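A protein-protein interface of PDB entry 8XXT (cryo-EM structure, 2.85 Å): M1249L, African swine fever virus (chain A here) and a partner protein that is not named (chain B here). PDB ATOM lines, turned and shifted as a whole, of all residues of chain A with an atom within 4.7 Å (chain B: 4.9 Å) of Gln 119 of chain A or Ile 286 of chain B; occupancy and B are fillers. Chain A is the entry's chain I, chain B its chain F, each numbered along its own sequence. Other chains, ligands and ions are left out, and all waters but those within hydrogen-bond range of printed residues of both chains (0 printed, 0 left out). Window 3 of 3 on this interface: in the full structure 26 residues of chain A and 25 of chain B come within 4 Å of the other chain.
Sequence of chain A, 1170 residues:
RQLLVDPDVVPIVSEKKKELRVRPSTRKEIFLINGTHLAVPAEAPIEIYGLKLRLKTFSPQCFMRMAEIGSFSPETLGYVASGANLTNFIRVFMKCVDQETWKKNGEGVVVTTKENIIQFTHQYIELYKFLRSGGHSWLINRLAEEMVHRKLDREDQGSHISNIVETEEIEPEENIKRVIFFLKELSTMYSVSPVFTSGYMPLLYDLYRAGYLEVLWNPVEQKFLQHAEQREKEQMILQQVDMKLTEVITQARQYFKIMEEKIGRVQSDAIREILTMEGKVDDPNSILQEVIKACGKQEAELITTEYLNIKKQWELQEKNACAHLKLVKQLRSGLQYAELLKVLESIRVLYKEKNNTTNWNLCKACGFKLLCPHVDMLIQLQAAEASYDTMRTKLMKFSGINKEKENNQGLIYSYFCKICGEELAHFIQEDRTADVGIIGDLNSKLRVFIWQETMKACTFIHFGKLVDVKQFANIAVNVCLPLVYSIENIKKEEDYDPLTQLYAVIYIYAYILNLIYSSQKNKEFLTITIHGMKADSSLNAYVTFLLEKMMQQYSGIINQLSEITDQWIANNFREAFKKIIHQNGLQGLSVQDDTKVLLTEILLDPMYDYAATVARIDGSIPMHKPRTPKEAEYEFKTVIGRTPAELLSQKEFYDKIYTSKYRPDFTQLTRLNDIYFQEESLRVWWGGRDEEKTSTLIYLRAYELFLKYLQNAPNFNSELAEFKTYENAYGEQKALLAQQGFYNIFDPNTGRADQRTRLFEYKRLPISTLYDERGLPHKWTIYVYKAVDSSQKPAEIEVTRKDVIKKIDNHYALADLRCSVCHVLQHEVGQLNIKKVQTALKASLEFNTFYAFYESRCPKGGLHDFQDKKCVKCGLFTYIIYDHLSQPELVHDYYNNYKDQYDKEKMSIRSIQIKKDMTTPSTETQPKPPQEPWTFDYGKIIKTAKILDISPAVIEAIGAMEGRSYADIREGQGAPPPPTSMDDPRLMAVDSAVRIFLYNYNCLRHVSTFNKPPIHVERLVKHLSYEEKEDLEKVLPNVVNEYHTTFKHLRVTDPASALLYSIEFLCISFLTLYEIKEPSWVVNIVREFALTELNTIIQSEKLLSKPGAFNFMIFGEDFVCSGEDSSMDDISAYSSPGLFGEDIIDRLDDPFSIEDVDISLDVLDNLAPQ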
ATOM      1  N   VAL A  92      29.538 -32.371   1.787  1.00  0.00           N
ATOM      2  CA  VAL A  92      29.265 -33.156   0.586  1.00  0.00           C
ATOM      3  C   VAL A  92      29.107 -32.243  -0.624  1.00  0.00           C
ATOM      4  O   VAL A  92      29.634 -32.526  -1.707  1.00  0.00           O
ATOM      5  CB  VAL A  92      28.024 -34.042   0.800  1.00  0.00           C
ATOM      6  CG1 VAL A  92      27.237 -34.186  -0.482  1.00  0.00           C
ATOM      7  CG2 VAL A  92      28.433 -35.405   1.331  1.00  0.00           C
ATOM      8  N   PHE A  93      28.394 -31.128  -0.458  1.00  0.00           N
ATOM      9  CA  PHE A  93      28.193 -30.211  -1.574  1.00  0.00           C
ATOM     10  C   PHE A  93      29.473 -29.463  -1.926  1.00  0.00           C
ATOM     11  O   PHE A  93      29.716 -29.167  -3.100  1.00  0.00           O
ATOM     12  CB  PHE A  93      27.081 -29.216  -1.247  1.00  0.00           C
ATOM     13  CG  PHE A  93      25.698 -29.722  -1.541  1.00  0.00           C
ATOM     14  CD1 PHE A  93      25.106 -30.676  -0.736  1.00  0.00           C
ATOM     15  CD2 PHE A  93      24.986 -29.233  -2.621  1.00  0.00           C
ATOM     16  CE1 PHE A  93      23.831 -31.131  -0.998  1.00  0.00           C
ATOM     17  CE2 PHE A  93      23.712 -29.687  -2.890  1.00  0.00           C
ATOM     18  CZ  PHE A  93      23.134 -30.637  -2.077  1.00  0.00           C
ATOM     19  N   CYS A  96      33.326 -31.269  -3.319  1.00  0.00           N
ATOM     20  CA  CYS A  96      33.360 -31.579  -4.742  1.00  0.00           C
ATOM     21  C   CYS A  96      34.034 -30.481  -5.551  1.00  0.00           C
ATOM     22  O   CYS A  96      34.586 -30.760  -6.620  1.00  0.00           O
ATOM     23  CB  CYS A  96      31.939 -31.803  -5.259  1.00  0.00           C
ATOM     24  SG  CYS A  96      31.131 -30.297  -5.843  1.00  0.00           S
ATOM     25  N   VAL A  97      33.992 -29.239  -5.069  1.00  0.00           N
ATOM     26  CA  VAL A  97      34.626 -28.134  -5.777  1.00  0.00           C
ATOM     27  C   VAL A  97      36.140 -28.145  -5.574  1.00  0.00           C
ATOM     28  O   VAL A  97      36.890 -27.741  -6.471  1.00  0.00           O
ATOM     29  CB  VAL A  97      33.986 -26.809  -5.329  1.00  0.00           C
ATOM     30  CG1 VAL A  97      34.996 -25.678  -5.332  1.00  0.00           C
ATOM     31  CG2 VAL A  97      32.797 -26.473  -6.216  1.00  0.00           C
ATOM     32  N   GLU A 115      35.506 -20.106 -13.366  1.00  0.00           N
ATOM     33  CA  GLU A 115      34.583 -21.227 -13.498  1.00  0.00           C
ATOM     34  C   GLU A 115      34.399 -21.948 -12.168  1.00  0.00           C
ATOM     35  O   GLU A 115      33.301 -22.432 -11.875  1.00  0.00           O
ATOM     36  CB  GLU A 115      35.058 -22.190 -14.593  1.00  0.00           C
ATOM     37  CG  GLU A 115      35.950 -23.336 -14.138  1.00  0.00           C
ATOM     38  CD  GLU A 115      37.355 -22.890 -13.796  1.00  0.00           C
ATOM     39  OE1 GLU A 115      37.753 -21.787 -14.225  1.00  0.00           O
ATOM     40  OE2 GLU A 115      38.063 -23.641 -13.094  1.00  0.00           O
ATOM     41  N   ASN A 116      35.448 -22.003 -11.341  1.00  0.00           N
ATOM     42  CA  ASN A 116      35.284 -22.537  -9.995  1.00  0.00           C
ATOM     43  C   ASN A 116      34.385 -21.647  -9.153  1.00  0.00           C
ATOM     44  O   ASN A 116      33.617 -22.152  -8.332  1.00  0.00           O
ATOM     45  CB  ASN A 116      36.641 -22.712  -9.316  1.00  0.00           C
ATOM     46  CG  ASN A 116      37.333 -23.987  -9.729  1.00  0.00           C
ATOM     47  OD1 ASN A 116      38.439 -23.961 -10.264  1.00  0.00           O
ATOM     48  ND2 ASN A 116      36.681 -25.118  -9.485  1.00  0.00           N
ATOM     49  N   ILE A 117      34.459 -20.329  -9.345  1.00  0.00           N
ATOM     50  CA  ILE A 117      33.549 -19.426  -8.647  1.00  0.00           C
ATOM     51  C   ILE A 117      32.107 -19.695  -9.063  1.00  0.00           C
ATOM     52  O   ILE A 117      31.195 -19.715  -8.225  1.00  0.00           O
ATOM     53  CB  ILE A 117      33.956 -17.963  -8.901  1.00  0.00           C
ATOM     54  CG1 ILE A 117      35.011 -17.521  -7.886  1.00  0.00           C
ATOM     55  CG2 ILE A 117      32.747 -17.045  -8.849  1.00  0.00           C
ATOM     56  CD1 ILE A 117      35.618 -16.171  -8.181  1.00  0.00           C
ATOM     57  N   ILE A 118      31.877 -19.900 -10.363  1.00  0.00           N
ATOM     58  CA  ILE A 118      30.525 -20.175 -10.845  1.00  0.00           C
ATOM     59  C   ILE A 118      30.018 -21.500 -10.290  1.00  0.00           C
ATOM     60  O   ILE A 118      28.860 -21.613  -9.860  1.00  0.00           O
ATOM     61  CB  ILE A 118      30.490 -20.151 -12.384  1.00  0.00           C
ATOM     62  CG1 ILE A 118      30.897 -18.771 -12.900  1.00  0.00           C
ATOM     63  CG2 ILE A 118      29.106 -20.527 -12.892  1.00  0.00           C
ATOM     64  CD1 ILE A 118      30.043 -17.645 -12.361  1.00  0.00           C
ATOM     65  N   GLN A 119      30.872 -22.525 -10.291  1.00  0.00           N
ATOM     66  CA  GLN A 119      30.477 -23.802  -9.707  1.00  0.00           C
ATOM     67  C   GLN A 119      30.190 -23.648  -8.221  1.00  0.00           C
ATOM     68  O   GLN A 119      29.242 -24.245  -7.699  1.00  0.00           O
ATOM     69  CB  GLN A 119      31.568 -24.849  -9.939  1.00  0.00           C
ATOM     70  CG  GLN A 119      31.057 -26.269 -10.203  1.00  0.00           C
ATOM     71  CD  GLN A 119      29.767 -26.327 -11.018  1.00  0.00           C
ATOM     72  OE1 GLN A 119      29.570 -25.560 -11.963  1.00  0.00           O
ATOM     73  NE2 GLN A 119      28.879 -27.239 -10.644  1.00  0.00           N
ATOM     74  N   PHE A 120      30.990 -22.833  -7.532  1.00  0.00           N
ATOM     75  CA  PHE A 120      30.785 -22.579  -6.112  1.00  0.00           C
ATOM     76  C   PHE A 120      29.418 -21.962  -5.856  1.00  0.00           C
ATOM     77  O   PHE A 120      28.680 -22.415  -4.976  1.00  0.00           O
ATOM     78  CB  PHE A 120      31.899 -21.665  -5.597  1.00  0.00           C
ATOM     79  CG  PHE A 120      31.994 -21.593  -4.101  1.00  0.00           C
ATOM     80  CD1 PHE A 120      31.111 -20.817  -3.371  1.00  0.00           C
ATOM     81  CD2 PHE A 120      32.981 -22.288  -3.426  1.00  0.00           C
ATOM     82  CE1 PHE A 120      31.203 -20.745  -2.000  1.00  0.00           C
ATOM     83  CE2 PHE A 120      33.079 -22.219  -2.052  1.00  0.00           C
ATOM     84  CZ  PHE A 120      32.187 -21.445  -1.341  1.00  0.00           C
ATOM     85  N   THR A 121      29.061 -20.920  -6.611  1.00  0.00           N
ATOM     86  CA  THR A 121      27.787 -20.255  -6.345  1.00  0.00           C
ATOM     87  C   THR A 121      26.607 -21.142  -6.727  1.00  0.00           C
ATOM     88  O   THR A 121      25.582 -21.147  -6.034  1.00  0.00           O
ATOM     89  CB  THR A 121      27.698 -18.904  -7.059  1.00  0.00           C
ATOM     90  OG1 THR A 121      26.337 -18.453  -7.045  1.00  0.00           O
ATOM     91  CG2 THR A 121      28.147 -19.007  -8.488  1.00  0.00           C
ATOM     92  N   HIS A 122      26.729 -21.907  -7.816  1.00  0.00           N
ATOM     93  CA  HIS A 122      25.659 -22.833  -8.172  1.00  0.00           C
ATOM     94  C   HIS A 122      25.478 -23.898  -7.095  1.00  0.00           C
ATOM     95  O   HIS A 122      24.348 -24.214  -6.697  1.00  0.00           O
ATOM     96  CB  HIS A 122      25.946 -23.477  -9.528  1.00  0.00           C
ATOM     97  CG  HIS A 122      24.971 -24.549  -9.901  1.00  0.00           C
ATOM     98  ND1 HIS A 122      23.618 -24.316 -10.021  1.00  0.00           N
ATOM     99  CD2 HIS A 122      25.151 -25.864 -10.168  1.00  0.00           C
ATOM    100  CE1 HIS A 122      23.009 -25.440 -10.353  1.00  0.00           C
ATOM    101  NE2 HIS A 122      23.916 -26.394 -10.448  1.00  0.00           N
ATOM    102  N   GLN A 123      26.588 -24.459  -6.605  1.00  0.00           N
ATOM    103  CA  GLN A 123      26.518 -25.457  -5.546  1.00  0.00           C
ATOM    104  C   GLN A 123      25.940 -24.867  -4.269  1.00  0.00           C
ATOM    105  O   GLN A 123      25.180 -25.531  -3.561  1.00  0.00           O
ATOM    106  CB  GLN A 123      27.905 -26.040  -5.281  1.00  0.00           C
ATOM    107  CG  GLN A 123      28.291 -27.179  -6.205  1.00  0.00           C
ATOM    108  CD  GLN A 123      27.575 -28.469  -5.867  1.00  0.00           C
ATOM    109  OE1 GLN A 123      26.659 -28.889  -6.574  1.00  0.00           O
ATOM    110  NE2 GLN A 123      27.986 -29.106  -4.778  1.00  0.00           N
ATOM    111  N   HIS B 165      23.820 -35.385 -10.043  1.00  0.00           N
ATOM    112  CA  HIS B 165      25.072 -36.100 -10.257  1.00  0.00           C
ATOM    113  C   HIS B 165      25.628 -36.534  -8.908  1.00  0.00           C
ATOM    114  O   HIS B 165      25.998 -35.693  -8.083  1.00  0.00           O
ATOM    115  CB  HIS B 165      26.083 -35.232 -11.006  1.00  0.00           C
ATOM    116  CG  HIS B 165      27.441 -35.850 -11.120  1.00  0.00           C
ATOM    117  ND1 HIS B 165      27.642 -37.118 -11.619  1.00  0.00           N
ATOM    118  CD2 HIS B 165      28.669 -35.373 -10.803  1.00  0.00           C
ATOM    119  CE1 HIS B 165      28.933 -37.397 -11.603  1.00  0.00           C
ATOM    120  NE2 HIS B 165      29.578 -36.355 -11.113  1.00  0.00           N
ATOM    121  N   GLN B 167      28.271 -38.464  -6.309  1.00  0.00           N
ATOM    122  CA  GLN B 167      29.678 -38.803  -6.148  1.00  0.00           C
ATOM    123  C   GLN B 167      29.969 -39.476  -4.812  1.00  0.00           C
ATOM    124  O   GLN B 167      31.144 -39.651  -4.466  1.00  0.00           O
ATOM    125  CB  GLN B 167      30.557 -37.558  -6.304  1.00  0.00           C
ATOM    126  CG  GLN B 167      30.561 -36.975  -7.702  1.00  0.00           C
ATOM    127  CD  GLN B 167      31.795 -36.145  -7.976  1.00  0.00           C
ATOM    128  OE1 GLN B 167      32.595 -35.885  -7.078  1.00  0.00           O
ATOM    129  NE2 GLN B 167      31.954 -35.717  -9.221  1.00  0.00           N
ATOM    130  N   PRO B 284      24.138 -30.040 -13.702  1.00  0.00           N
ATOM    131  CA  PRO B 284      24.056 -31.136 -12.731  1.00  0.00           C
ATOM    132  C   PRO B 284      24.647 -30.738 -11.388  1.00  0.00           C
ATOM    133  O   PRO B 284      25.643 -30.016 -11.312  1.00  0.00           O
ATOM    134  CB  PRO B 284      24.874 -32.259 -13.382  1.00  0.00           C
ATOM    135  CG  PRO B 284      25.052 -31.874 -14.816  1.00  0.00           C
ATOM    136  CD  PRO B 284      24.462 -30.517 -15.055  1.00  0.00           C
ATOM    137  N   ILE B 285      24.016 -31.222 -10.324  1.00  0.00           N
ATOM    138  CA  ILE B 285      24.413 -30.907  -8.959  1.00  0.00           C
ATOM    139  C   ILE B 285      25.222 -32.066  -8.399  1.00  0.00           C
ATOM    140  O   ILE B 285      24.812 -33.228  -8.497  1.00  0.00           O
ATOM    141  CB  ILE B 285      23.181 -30.618  -8.089  1.00  0.00           C
ATOM    142  CG1 ILE B 285      22.190 -29.757  -8.869  1.00  0.00           C
ATOM    143  CG2 ILE B 285      23.593 -29.935  -6.800  1.00  0.00           C
ATOM    144  CD1 ILE B 285      20.776 -29.875  -8.390  1.00  0.00           C
ATOM    145  N   ILE B 286      26.366 -31.749  -7.801  1.00  0.00           N
ATOM    146  CA  ILE B 286      27.346 -32.739  -7.371  1.00  0.00           C
ATOM    147  C   ILE B 286      27.193 -32.908  -5.864  1.00  0.00           C
ATOM    148  O   ILE B 286      27.682 -32.086  -5.085  1.00  0.00           O
ATOM    149  CB  ILE B 286      28.771 -32.318  -7.743  1.00  0.00           C
ATOM    150  CG1 ILE B 286      28.805 -31.637  -9.115  1.00  0.00           C
ATOM    151  CG2 ILE B 286      29.703 -33.510  -7.721  1.00  0.00           C
ATOM    152  CD1 ILE B 286      28.746 -30.125  -9.054  1.00  0.00           C
ATOM    153  N   CYS B 287      26.537 -33.986  -5.443  1.00  0.00           N
ATOM    154  CA  CYS B 287      26.340 -34.262  -4.024  1.00  0.00           C
ATOM    155  C   CYS B 287      25.982 -35.738  -3.851  1.00  0.00           C
ATOM    156  O   CYS B 287      25.870 -36.486  -4.826  1.00  0.00           O
ATOM    157  CB  CYS B 287      25.305 -33.299  -3.428  1.00  0.00           C
ATOM    158  SG  CYS B 287      23.834 -33.005  -4.421  1.00  0.00           S
ATOM    159  N   SER B 288      25.803 -36.155  -2.597  1.00  0.00           N
ATOM    160  CA  SER B 288      25.761 -37.560  -2.215  1.00  0.00           C
ATOM    161  C   SER B 288      24.411 -38.193  -2.535  1.00  0.00           C
ATOM    162  O   SER B 288      23.393 -37.515  -2.666  1.00  0.00           O
ATOM    163  CB  SER B 288      26.033 -37.718  -0.721  1.00  0.00           C
ATOM    164  OG  SER B 288      24.865 -37.434   0.031  1.00  0.00           O
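O of Ile 286 of chain B lies within hydrogen-bond range of NE2 of Gln 123 of chain A (3.0 Å).
SG of Cys 96 of chain A lies within hydrogen-bond range of NE2 of Gln 123 of chain A (3.5 Å). The backbone carbonyl oxygen (O) of Cys 287 of chain B is in hydrogen-bond range of the backbone NH (N) of Gln 167 of chain B. The backbone carbonyl oxygen (O) of Ile 285 of chain B lies within hydrogen-bond range of the backbone NH (N) of His 165 of chain B, 2.8 Å away. The backbone carbonyl oxygen of Phe 93 of chain A is in hydrogen-bond range of the side-chain amide nitrogen of Gln 123 of chain A. The backbone NH of Cys 287 of chain B sits at hydrogen-bond distance from the backbone carbonyl oxygen of His 165 of chain B (3.2 Å). The backbone carbonyl oxygen of Phe 93 of chain A is in hydrogen-bond range of the side-chain sulfur of Cys 96 of chain A, 3.3 Å away.
Of the 13 printed residues of chain A, 5 touch a printed residue of chain B. Hydrophobic or aromatic side chains of chain A that line the printed part of chain B: Val 92 and Phe 93. Of the 7 printed residues of chain B, 4 touch a printed residue of chain A. Hydrophobic or aromatic side chains of chain B that line the printed part of chain A: Ile 285 and Ile 286. Among the printed residues, 9 pairs touch across the chains.
Of chain B, only Ile 286 (3.3 Å) comes within 4 Å of Gln 119 of chain A. Printed residues of chain A within 4 Å of Ile 286 of chain B: Val 92, Cys 96, Gln 119 and Gln 123. Of the printed residues of chain B, Phe 93 of chain A touches Ile 285 and Cys 287. Printed residues of chain A within 4 Å of Ser 288 of chain B: Val 92 (3.2 Å). Of the printed residues of chain A, Ile 285 of chain B touches Phe 93 and Gln 123. The nearest residue of chain B that does not touch Gln 119 of chain A is Pro 284 of chain B (4.3 Å). The nearest printed residue of chain A that does not touch Ile 286 of chain B is Phe 93 of chain A (4.01 Å). The nearest printed residue of chain B that does not touch Phe 93 of chain A is Ile 286 of chain B (4.01 Å).
O of Ile 286 of chain B touches O of Val 92 of chain A (3.9 Å). CB of Cys 287 of chain B touches CG1 of Val 92 of chain A (3.6 Å). Val 92 of chain A touches Ser 288 of chain B. Phe 93 of chain A touches Ile 285 of chain B (CE2 to CG2, 3.9 Å). Phe 93 of chain A touches Cys 287 of chain B. SG of Cys 96 of chain A touches CB of Ile 286 of chain B, 3.6 Å away. Gln 119 of chain A touches Ile 286 of chain B. Gln 123 of chain A touches Ile 285 of chain B (OE1 to CG2, 3.2 Å).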
